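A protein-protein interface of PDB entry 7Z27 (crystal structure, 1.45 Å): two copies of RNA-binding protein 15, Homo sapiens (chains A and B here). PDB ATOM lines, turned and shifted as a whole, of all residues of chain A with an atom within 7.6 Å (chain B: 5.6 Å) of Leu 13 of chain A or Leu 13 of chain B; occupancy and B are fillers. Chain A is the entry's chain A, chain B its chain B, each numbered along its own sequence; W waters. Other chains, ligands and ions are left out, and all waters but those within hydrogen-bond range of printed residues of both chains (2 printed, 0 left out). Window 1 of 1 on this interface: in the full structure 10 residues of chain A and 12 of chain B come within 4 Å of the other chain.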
ATOM      1  N   SER A  10     -37.491 -14.944  -9.961  1.00  0.00           N
ATOM      2  CA  SER A  10     -36.075 -15.226  -9.751  1.00  0.00           C
ATOM      3  C   SER A  10     -35.340 -13.895  -9.620  1.00  0.00           C
ATOM      4  O   SER A  10     -35.623 -12.957 -10.365  1.00  0.00           O
ATOM      5  CB  SER A  10     -35.522 -16.034 -10.928  1.00  0.00           C
ATOM      6  OG  SER A  10     -34.265 -16.644 -10.647  1.00  0.00           O
ATOM      7  N   PRO A  11     -34.389 -13.812  -8.690  1.00  0.00           N
ATOM      8  CA  PRO A  11     -33.682 -12.542  -8.481  1.00  0.00           C
ATOM      9  C   PRO A  11     -32.922 -12.108  -9.727  1.00  0.00           C
ATOM     10  O   PRO A  11     -32.278 -12.915 -10.406  1.00  0.00           O
ATOM     11  CB  PRO A  11     -32.738 -12.848  -7.311  1.00  0.00           C
ATOM     12  CG  PRO A  11     -32.552 -14.340  -7.357  1.00  0.00           C
ATOM     13  CD  PRO A  11     -33.888 -14.873  -7.801  1.00  0.00           C
ATOM     14  N   LYS A  12     -33.003 -10.808 -10.015  1.00  0.00           N
ATOM     15  CA  LYS A  12     -32.376 -10.278 -11.218  1.00  0.00           C
ATOM     16  C   LYS A  12     -30.860 -10.305 -11.102  1.00  0.00           C
ATOM     17  O   LYS A  12     -30.167 -10.523 -12.099  1.00  0.00           O
ATOM     18  CB  LYS A  12     -32.863  -8.855 -11.484  1.00  0.00           C
ATOM     19  CG  LYS A  12     -34.249  -8.770 -12.106  1.00  0.00           C
ATOM     20  CD  LYS A  12     -34.355  -7.587 -13.063  1.00  0.00           C
ATOM     21  CE  LYS A  12     -33.784  -7.911 -14.445  1.00  0.00           C
ATOM     22  NZ  LYS A  12     -33.390  -6.665 -15.163  1.00  0.00           N
ATOM     23  N   LEU A  13     -30.325 -10.083  -9.898  1.00  0.00           N
ATOM     24  CA  LEU A  13     -28.891 -10.090  -9.606  1.00  0.00           C
ATOM     25  C   LEU A  13     -28.115  -8.961 -10.281  1.00  0.00           C
ATOM     26  O   LEU A  13     -26.877  -9.006 -10.306  1.00  0.00           O
ATOM     27  CB  LEU A  13     -28.236 -11.456  -9.848  1.00  0.00           C
ATOM     28  CG  LEU A  13     -28.823 -12.589  -9.007  1.00  0.00           C
ATOM     29  CD1 LEU A  13     -28.073 -13.882  -9.263  1.00  0.00           C
ATOM     30  CD2 LEU A  13     -28.788 -12.246  -7.507  1.00  0.00           C
ATOM     31  N   CYS A  14     -28.805  -7.944 -10.803  1.00  0.00           N
ATOM     32  CA  CYS A  14     -28.160  -6.746 -11.334  1.00  0.00           C
ATOM     33  C   CYS A  14     -27.116  -6.239 -10.351  1.00  0.00           C
ATOM     34  O   CYS A  14     -27.369  -6.170  -9.145  1.00  0.00           O
ATOM     35  CB  CYS A  14     -29.208  -5.639 -11.442  1.00  0.00           C
ATOM     36  SG  CYS A  14     -30.481  -5.864 -12.682  1.00  0.00           S
ATOM     37  N   LEU A  15     -25.952  -5.847 -10.870  1.00  0.00           N
ATOM     38  CA  LEU A  15     -24.904  -5.238 -10.049  1.00  0.00           C
ATOM     39  C   LEU A  15     -25.284  -3.791  -9.768  1.00  0.00           C
ATOM     40  O   LEU A  15     -24.949  -2.878 -10.525  1.00  0.00           O
ATOM     41  CB  LEU A  15     -23.561  -5.324 -10.761  1.00  0.00           C
ATOM     42  CG  LEU A  15     -22.304  -4.963  -9.966  1.00  0.00           C
ATOM     43  CD1 LEU A  15     -22.199  -5.761  -8.665  1.00  0.00           C
ATOM     44  CD2 LEU A  15     -21.069  -5.178 -10.832  1.00  0.00           C
ATOM     45  N   ALA A  16     -25.972  -3.570  -8.647  1.00  0.00           N
ATOM     46  CA  ALA A  16     -26.559  -2.263  -8.362  1.00  0.00           C
ATOM     47  C   ALA A  16     -25.561  -1.278  -7.768  1.00  0.00           C
ATOM     48  O   ALA A  16     -25.743  -0.065  -7.920  1.00  0.00           O
ATOM     49  CB  ALA A  16     -27.749  -2.422  -7.419  1.00  0.00           C
ATOM     50  N   ASN A  31     -19.702  -5.775  -3.386  1.00  0.00           N
ATOM     51  CA  ASN A  31     -20.552  -5.690  -4.567  1.00  0.00           C
ATOM     52  C   ASN A  31     -21.973  -6.033  -4.151  1.00  0.00           C
ATOM     53  O   ASN A  31     -22.193  -7.012  -3.424  1.00  0.00           O
ATOM     54  CB  ASN A  31     -20.102  -6.699  -5.625  1.00  0.00           C
ATOM     55  CG  ASN A  31     -18.708  -6.419  -6.146  1.00  0.00           C
ATOM     56  OD1 ASN A  31     -18.238  -5.284  -6.124  1.00  0.00           O
ATOM     57  ND2 ASN A  31     -18.030  -7.464  -6.602  1.00  0.00           N
ATOM     58  N   MET A  32     -22.949  -5.258  -4.616  1.00  0.00           N
ATOM     59  CA  MET A  32     -24.320  -5.451  -4.171  1.00  0.00           C
ATOM     60  C   MET A  32     -25.192  -5.820  -5.359  1.00  0.00           C
ATOM     61  O   MET A  32     -25.222  -5.092  -6.358  1.00  0.00           O
ATOM     62  CB  MET A  32     -24.807  -4.197  -3.454  1.00  0.00           C
ATOM     63  CG  MET A  32     -24.003  -4.063  -2.173  1.00  0.00           C
ATOM     64  SD  MET A  32     -24.417  -2.776  -1.014  1.00  0.00           S
ATOM     65  CE  MET A  32     -25.864  -2.232  -1.755  1.00  0.00           C
ATOM     66  N   HIS A  33     -25.882  -6.958  -5.256  1.00  0.00           N
ATOM     67  CA  HIS A  33     -26.703  -7.505  -6.333  1.00  0.00           C
ATOM     68  C   HIS A  33     -28.180  -7.448  -5.971  1.00  0.00           C
ATOM     69  O   HIS A  33     -28.565  -7.753  -4.843  1.00  0.00           O
ATOM     70  CB  HIS A  33     -26.335  -8.965  -6.593  1.00  0.00           C
ATOM     71  CG  HIS A  33     -24.928  -9.158  -7.056  1.00  0.00           C
ATOM     72  ND1 HIS A  33     -24.598  -9.292  -8.391  1.00  0.00           N
ATOM     73  CD2 HIS A  33     -23.767  -9.275  -6.366  1.00  0.00           C
ATOM     74  CE1 HIS A  33     -23.292  -9.460  -8.501  1.00  0.00           C
ATOM     75  NE2 HIS A  33     -22.764  -9.456  -7.289  1.00  0.00           N
ATOM     76  N   LEU A  34     -29.015  -7.098  -6.945  1.00  0.00           N
ATOM     77  CA  LEU A  34     -30.440  -6.951  -6.676  1.00  0.00           C
ATOM     78  C   LEU A  34     -31.090  -8.314  -6.450  1.00  0.00           C
ATOM     79  O   LEU A  34     -30.954  -9.233  -7.271  1.00  0.00           O
ATOM     80  CB  LEU A  34     -31.122  -6.235  -7.845  1.00  0.00           C
ATOM     81  CG  LEU A  34     -32.627  -5.981  -7.714  1.00  0.00           C
ATOM     82  CD1 LEU A  34     -32.942  -5.005  -6.588  1.00  0.00           C
ATOM     83  CD2 LEU A  34     -33.158  -5.450  -9.028  1.00  0.00           C
ATOM     84  N   LEU A  35     -31.811  -8.444  -5.333  1.00  0.00           N
ATOM     85  CA  LEU A  35     -32.581  -9.646  -5.042  1.00  0.00           C
ATOM     86  C   LEU A  35     -34.061  -9.460  -5.342  1.00  0.00           C
ATOM     87  O   LEU A  35     -34.673 -10.306  -5.999  1.00  0.00           O
ATOM     88  CB  LEU A  35     -32.401 -10.073  -3.578  1.00  0.00           C
ATOM     89  CG  LEU A  35     -31.015 -10.570  -3.192  1.00  0.00           C
ATOM     90  CD1 LEU A  35     -30.979 -10.821  -1.696  1.00  0.00           C
ATOM     91  CD2 LEU A  35     -30.644 -11.844  -3.946  1.00  0.00           C
ATOM     92  N   GLN A  36     -34.654  -8.368  -4.866  1.00  0.00           N
ATOM     93  CA  GLN A  36     -36.060  -8.109  -5.126  1.00  0.00           C
ATOM     94  C   GLN A  36     -36.342  -6.641  -4.861  1.00  0.00           C
ATOM     95  O   GLN A  36     -35.476  -5.889  -4.404  1.00  0.00           O
ATOM     96  CB  GLN A  36     -36.968  -9.021  -4.300  1.00  0.00           C
ATOM     97  CG  GLN A  36     -36.890  -8.791  -2.809  1.00  0.00           C
ATOM     98  CD  GLN A  36     -38.059  -9.432  -2.082  1.00  0.00           C
ATOM     99  OE1 GLN A  36     -39.159  -8.888  -2.069  1.00  0.00           O
ATOM    100  NE2 GLN A  36     -37.828 -10.590  -1.483  1.00  0.00           N
ATOM    101  N   LEU A  90     -28.142  -8.272  -2.173  1.00  0.00           N
ATOM    102  CA  LEU A  90     -27.182  -9.181  -1.563  1.00  0.00           C
ATOM    103  C   LEU A  90     -25.809  -8.528  -1.674  1.00  0.00           C
ATOM    104  O   LEU A  90     -25.336  -8.257  -2.789  1.00  0.00           O
ATOM    105  CB  LEU A  90     -27.174 -10.526  -2.288  1.00  0.00           C
ATOM    106  CG  LEU A  90     -26.253 -11.578  -1.679  1.00  0.00           C
ATOM    107  CD1 LEU A  90     -26.790 -12.014  -0.318  1.00  0.00           C
ATOM    108  CD2 LEU A  90     -26.146 -12.752  -2.623  1.00  0.00           C
ATOM    109  N   ASP A 163     -33.328 -17.106  -2.348  1.00  0.00           N
ATOM    110  CA  ASP A 163     -33.761 -18.297  -3.056  1.00  0.00           C
ATOM    111  C   ASP A 163     -32.539 -19.031  -3.608  1.00  0.00           C
ATOM    112  O   ASP A 163     -31.399 -18.584  -3.463  1.00  0.00           O
ATOM    113  CB  ASP A 163     -34.836 -17.956  -4.088  1.00  0.00           C
ATOM    114  CG  ASP A 163     -34.275 -17.304  -5.330  1.00  0.00           C
ATOM    115  OD1 ASP A 163     -34.929 -17.404  -6.390  1.00  0.00           O
ATOM    116  OD2 ASP A 163     -33.182 -16.704  -5.258  1.00  0.00           O
ATOM    117  N   PRO A 165     -30.987 -19.563  -6.601  1.00  0.00           N
ATOM    118  CA  PRO A 165     -29.932 -18.847  -7.335  1.00  0.00           C
ATOM    119  C   PRO A 165     -29.211 -17.801  -6.507  1.00  0.00           C
ATOM    120  O   PRO A 165     -28.025 -17.548  -6.748  1.00  0.00           O
ATOM    121  CB  PRO A 165     -30.655 -18.253  -8.555  1.00  0.00           C
ATOM    122  CG  PRO A 165     -32.094 -18.523  -8.376  1.00  0.00           C
ATOM    123  CD  PRO A 165     -32.335 -19.217  -7.080  1.00  0.00           C
ATOM    124  N   ALA A 166     -29.880 -17.208  -5.515  1.00  0.00           N
ATOM    125  CA  ALA A 166     -29.209 -16.243  -4.654  1.00  0.00           C
ATOM    126  C   ALA A 166     -28.146 -16.908  -3.788  1.00  0.00           C
ATOM    127  O   ALA A 166     -27.060 -16.348  -3.601  1.00  0.00           O
ATOM    128  CB  ALA A 166     -30.233 -15.509  -3.785  1.00  0.00           C
ATOM    129  N   LYS A 167     -28.435 -18.103  -3.257  1.00  0.00           N
ATOM    130  CA  LYS A 167     -27.471 -18.789  -2.397  1.00  0.00           C
ATOM    131  C   LYS A 167     -26.169 -19.104  -3.123  1.00  0.00           C
ATOM    132  O   LYS A 167     -25.102 -19.082  -2.505  1.00  0.00           O
ATOM    133  CB  LYS A 167     -28.058 -20.077  -1.811  1.00  0.00           C
ATOM    134  CG  LYS A 167     -29.522 -20.014  -1.441  1.00  0.00           C
ATOM    135  CD  LYS A 167     -29.945 -21.240  -0.645  1.00  0.00           C
ATOM    136  CE  LYS A 167     -31.265 -21.007   0.071  1.00  0.00           C
ATOM    137  NZ  LYS A 167     -31.153 -19.981   1.147  1.00  0.00           N
ATOM    138  N   ALA A 168     -26.232 -19.414  -4.421  1.00  0.00           N
ATOM    139  CA  ALA A 168     -25.007 -19.699  -5.163  1.00  0.00           C
ATOM    140  C   ALA A 168     -24.046 -18.519  -5.115  1.00  0.00           C
ATOM    141  O   ALA A 168     -22.826 -18.702  -5.024  1.00  0.00           O
ATOM    142  CB  ALA A 168     -25.341 -20.069  -6.608  1.00  0.00           C
ATOM    143  N   LEU A 169     -24.580 -17.296  -5.179  1.00  0.00           N
ATOM    144  CA  LEU A 169     -23.751 -16.112  -4.981  1.00  0.00           C
ATOM    145  C   LEU A 169     -23.251 -16.043  -3.547  1.00  0.00           C
ATOM    146  O   LEU A 169     -22.091 -15.696  -3.300  1.00  0.00           O
ATOM    147  CB  LEU A 169     -24.567 -14.856  -5.289  1.00  0.00           C
ATOM    148  CG  LEU A 169     -24.132 -13.927  -6.417  1.00  0.00           C
ATOM    149  CD1 LEU A 169     -25.027 -12.705  -6.447  1.00  0.00           C
ATOM    150  CD2 LEU A 169     -22.680 -13.526  -6.254  1.00  0.00           C
ATOM    151  N   PRO B  11     -26.572  -1.151 -15.015  1.00  0.00           N
ATOM    152  CA  PRO B  11     -25.800  -2.234 -14.412  1.00  0.00           C
ATOM    153  C   PRO B  11     -25.686  -3.521 -15.235  1.00  0.00           C
ATOM    154  O   PRO B  11     -26.616  -3.926 -15.929  1.00  0.00           O
ATOM    155  CB  PRO B  11     -26.563  -2.487 -13.087  1.00  0.00           C
ATOM    156  CG  PRO B  11     -27.542  -1.290 -12.948  1.00  0.00           C
ATOM    157  CD  PRO B  11     -27.000  -0.256 -13.936  1.00  0.00           C
ATOM    158  N   LYS B  12     -24.515  -4.142 -15.144  1.00  0.00           N
ATOM    159  CA  LYS B  12     -24.284  -5.468 -15.677  1.00  0.00           C
ATOM    160  C   LYS B  12     -24.897  -6.516 -14.757  1.00  0.00           C
ATOM    161  O   LYS B  12     -25.286  -6.240 -13.609  1.00  0.00           O
ATOM    162  CB  LYS B  12     -22.784  -5.739 -15.794  1.00  0.00           C
ATOM    163  N   LEU B  13     -24.959  -7.743 -15.270  1.00  0.00           N
ATOM    164  CA  LEU B  13     -25.333  -8.972 -14.590  1.00  0.00           C
ATOM    165  C   LEU B  13     -26.837  -9.156 -14.390  1.00  0.00           C
ATOM    166  O   LEU B  13     -27.222 -10.141 -13.745  1.00  0.00           O
ATOM    167  CB  LEU B  13     -24.569  -9.178 -13.275  1.00  0.00           C
ATOM    168  CG  LEU B  13     -23.047  -9.187 -13.420  1.00  0.00           C
ATOM    169  CD1 LEU B  13     -22.381  -9.471 -12.087  1.00  0.00           C
ATOM    170  CD2 LEU B  13     -22.595 -10.217 -14.451  1.00  0.00           C
ATOM    171  N   CYS B  14     -27.699  -8.270 -14.901  1.00  0.00           N
ATOM    172  CA  CYS B  14     -29.130  -8.551 -14.818  1.00  0.00           C
ATOM    173  C   CYS B  14     -29.568  -9.773 -15.595  1.00  0.00           C
ATOM    174  O   CYS B  14     -29.066 -10.064 -16.684  1.00  0.00           O
ATOM    175  CB  CYS B  14     -30.076  -7.367 -15.039  1.00  0.00           C
ATOM    176  SG  CYS B  14     -29.578  -5.747 -14.520  1.00  0.00           S
ATOM    177  N   LEU B  15     -30.513 -10.489 -14.999  1.00  0.00           N
ATOM    178  CA  LEU B  15     -31.165 -11.604 -15.663  1.00  0.00           C
ATOM    179  C   LEU B  15     -31.791 -11.117 -16.961  1.00  0.00           C
ATOM    180  O   LEU B  15     -32.573 -10.157 -16.972  1.00  0.00           O
ATOM    181  CB  LEU B  15     -32.237 -12.170 -14.733  1.00  0.00           C
ATOM    182  CG  LEU B  15     -33.004 -13.388 -15.239  1.00  0.00           C
ATOM    183  CD1 LEU B  15     -32.046 -14.566 -15.370  1.00  0.00           C
ATOM    184  CD2 LEU B  15     -34.136 -13.722 -14.281  1.00  0.00           C
ATOM    185  N   HIS B  33     -27.479 -14.177 -17.551  1.00  0.00           N
ATOM    186  CA  HIS B  33     -27.255 -12.819 -17.055  1.00  0.00           C
ATOM    187  C   HIS B  33     -26.304 -12.069 -17.985  1.00  0.00           C
ATOM    188  O   HIS B  33     -25.355 -12.652 -18.503  1.00  0.00           O
ATOM    189  CB  HIS B  33     -26.662 -12.885 -15.641  1.00  0.00           C
ATOM    190  CG  HIS B  33     -27.576 -13.522 -14.644  1.00  0.00           C
ATOM    191  ND1 HIS B  33     -28.340 -12.780 -13.768  1.00  0.00           N
ATOM    192  CD2 HIS B  33     -27.876 -14.822 -14.402  1.00  0.00           C
ATOM    193  CE1 HIS B  33     -29.052 -13.597 -13.010  1.00  0.00           C
ATOM    194  NE2 HIS B  33     -28.786 -14.839 -13.369  1.00  0.00           N
ATOM    195  N   LEU B  34     -26.544 -10.773 -18.192  1.00  0.00           N
ATOM    196  CA  LEU B  34     -25.773 -10.032 -19.188  1.00  0.00           C
ATOM    197  C   LEU B  34     -24.356  -9.755 -18.697  1.00  0.00           C
ATOM    198  O   LEU B  34     -24.162  -9.198 -17.613  1.00  0.00           O
ATOM    199  CB  LEU B  34     -26.468  -8.710 -19.503  1.00  0.00           C
ATOM    200  CG  LEU B  34     -25.833  -7.860 -20.601  1.00  0.00           C
ATOM    201  CD1 LEU B  34     -25.874  -8.568 -21.935  1.00  0.00           C
ATOM    202  CD2 LEU B  34     -26.585  -6.530 -20.647  1.00  0.00           C
ATOM    203  N   LEU B  35     -23.360 -10.132 -19.499  1.00  0.00           N
ATOM    204  CA  LEU B  35     -21.965  -9.825 -19.204  1.00  0.00           C
ATOM    205  C   LEU B  35     -21.462  -8.620 -19.984  1.00  0.00           C
ATOM    206  O   LEU B  35     -20.827  -7.729 -19.410  1.00  0.00           O
ATOM    207  CB  LEU B  35     -21.074 -11.031 -19.526  1.00  0.00           C
ATOM    208  CG  LEU B  35     -21.264 -12.277 -18.671  1.00  0.00           C
ATOM    209  CD1 LEU B  35     -20.426 -13.403 -19.216  1.00  0.00           C
ATOM    210  CD2 LEU B  35     -20.879 -11.982 -17.238  1.00  0.00           C
ATOM    211  N   ASP B 163     -15.448 -10.767 -15.462  1.00  0.00           N
ATOM    212  CA  ASP B 163     -14.716  -9.936 -14.519  1.00  0.00           C
ATOM    213  C   ASP B 163     -14.943 -10.461 -13.103  1.00  0.00           C
ATOM    214  O   ASP B 163     -15.614 -11.474 -12.900  1.00  0.00           O
ATOM    215  CB  ASP B 163     -15.048  -8.457 -14.727  1.00  0.00           C
ATOM    216  CG  ASP B 163     -16.499  -8.110 -14.405  1.00  0.00           C
ATOM    217  OD1 ASP B 163     -17.274  -8.990 -13.987  1.00  0.00           O
ATOM    218  OD2 ASP B 163     -16.865  -6.924 -14.564  1.00  0.00           O
ATOM    219  N   PRO B 165     -16.784  -9.368 -10.426  1.00  0.00           N
ATOM    220  CA  PRO B 165     -18.184  -9.543  -9.999  1.00  0.00           C
ATOM    221  C   PRO B 165     -18.880 -10.696 -10.691  1.00  0.00           C
ATOM    222  O   PRO B 165     -19.639 -11.442 -10.059  1.00  0.00           O
ATOM    223  CB  PRO B 165     -18.828  -8.194 -10.338  1.00  0.00           C
ATOM    224  CG  PRO B 165     -17.701  -7.225 -10.307  1.00  0.00           C
ATOM    225  CD  PRO B 165     -16.529  -7.987 -10.869  1.00  0.00           C
ATOM    226  N   ALA B 166     -18.631 -10.873 -11.988  1.00  0.00           N
ATOM    227  CA  ALA B 166     -19.254 -11.973 -12.709  1.00  0.00           C
ATOM    228  C   ALA B 166     -18.746 -13.329 -12.230  1.00  0.00           C
ATOM    229  O   ALA B 166     -19.515 -14.296 -12.180  1.00  0.00           O
ATOM    230  CB  ALA B 166     -19.010 -11.805 -14.205  1.00  0.00           C
ATOM    231  N   LEU B 169     -20.903 -15.020  -9.644  1.00  0.00           N
ATOM    232  CA  LEU B 169     -22.101 -15.712 -10.091  1.00  0.00           C
ATOM    233  C   LEU B 169     -21.752 -17.055 -10.705  1.00  0.00           C
ATOM    234  O   LEU B 169     -22.567 -17.982 -10.673  1.00  0.00           O
ATOM    235  CB  LEU B 169     -22.814 -14.872 -11.151  1.00  0.00           C
ATOM    236  CG  LEU B 169     -23.933 -13.899 -10.796  1.00  0.00           C
ATOM    237  CD1 LEU B 169     -23.359 -12.631 -10.192  1.00  0.00           C
ATOM    238  CD2 LEU B 169     -24.715 -13.583 -12.060  1.00  0.00           C
HETATM  239  O   HOH W   1     -32.430  -3.719 -15.297  1.00  0.00           O
HETATM  240  O   HOH W   2     -19.986 -10.071  -7.284  1.00  0.00           O
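N of Leu 15 of chain B lies within hydrogen-bond range of O of Lys 12 of chain A.
The backbone carbonyl oxygen (O) of Lys 12 of chain A lies close to the backbone carbonyl oxygen (O) of Leu 13 of chain B, at 3.4 Å.
SG of Cys 14 of chain B is disulfide-bonded to SG of Cys 14 of chain A.
O of Lys 12 of chain A lies within hydrogen-bond range of ND1 of His 33 of chain B, at 3.3 Å.
The backbone carbonyl oxygen of Lys 12 of chain B sits at hydrogen-bond distance from the backbone NH of Leu 15 of chain A (2.8 Å).
O of Leu 13 of chain B is in hydrogen-bond range of ND1 of His 33 of chain B, 2.9 Å away.
N of Leu 90 of chain A sits at hydrogen-bond distance from O of His 33 of chain A, at 2.8 Å.
The backbone NH (N) of Leu 13 of chain B is in hydrogen-bond range of the backbone carbonyl oxygen (O) of Leu 34 of chain B (2.9 Å).
A ring nitrogen (ND1) of His 33 of chain A lies within hydrogen-bond range of the backbone carbonyl oxygen (O) of Leu 13 of chain A (3.0 Å).
O of Cys 14 of chain A lies within hydrogen-bond range of N of Leu 34 of chain A (2.9 Å).
The backbone carbonyl oxygen (O) of Leu 34 of chain A lies within hydrogen-bond range of the backbone NH (N) of Leu 13 of chain A, 2.8 Å away.
Among the printed residues, merely in contact across the chains: Leu 15 of chain A with Pro 11 of chain B, Lys 12 of chain A with Cys 14 of chain B, His 33 of chain A with Leu 169 of chain B, Leu 13 of chain A with Leu 13 of chain B, His 33 of chain A with Leu 13 of chain B, Cys 14 of chain A with Lys 12 of chain B, Asn 31 of chain A with Pro 165 of chain B, Leu 15 of chain A with Pro 165 of chain B, Leu 13 of chain A with His 33 of chain B and Cys 14 of chain A with Leu 13 of chain B.
Leu 13 of chain A touches just these residues of chain B: Leu 13 (3.6 Å) and His 33 (3.9 Å).
Printed residues of chain B within 4 Å of Leu 15 of chain A: Pro 11, Lys 12 and Pro 165.
Of the printed residues of chain B, His 33 of chain A touches Leu 13 and Leu 169.
Gln 36 of chain A touches none of the printed residues of chain B.
Of the printed residues of chain A, Leu 13 of chain B touches Lys 12, Leu 13, Cys 14 and His 33.
Printed residues of chain A within 4 Å of His 33 of chain B: Lys 12 and Leu 13.
Of the 20 printed residues of chain A, 6 touch a printed residue of chain B.
Hydrophobic or aromatic side chains of chain A within 4 Å of the printed part of chain B: Leu 13, Leu 15 and His 33.
Among the printed residues, 15 pairs touch across the chains.
Among the printed residues, no Asp or Glu carboxylate lies within 4 Å of a Lys or Arg side-chain nitrogen of the other chain.
Lys 12 of chain A touches Cys 14 of chain B, and with the chains exchanged Cys 14 of chain A touches Lys 12 of chain B.
Lys 12 of chain A touches His 33 of chain B, but with the chains exchanged His 33 of chain A does not touch Lys 12 of chain B (6.1 Å).
Leu 13 of chain A touches His 33 of chain B, and with the chains exchanged His 33 of chain A touches Leu 13 of chain B.
His 33 of chain A touches Leu 169 of chain B, but with the chains exchanged Leu 169 of chain A does not touch His 33 of chain B (7.8 Å).
12 positions are printed for both chains.
Of the 15 pairs that touch across the chains among the printed residues, 8 have their exchanged pair printed and touching as well.
Water W2 lies within hydrogen-bond range of a ring nitrogen (NE2) of His 33 of chain A (2.8 Å), the backbone carbonyl oxygen of Pro 165 of chain B (3.1 Å) and the side-chain amide nitrogen of Asn 31 of chain A (3.3 Å).
Water W1 bridges NZ of Lys 12 of chain A and SG of Cys 14 of chain B.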
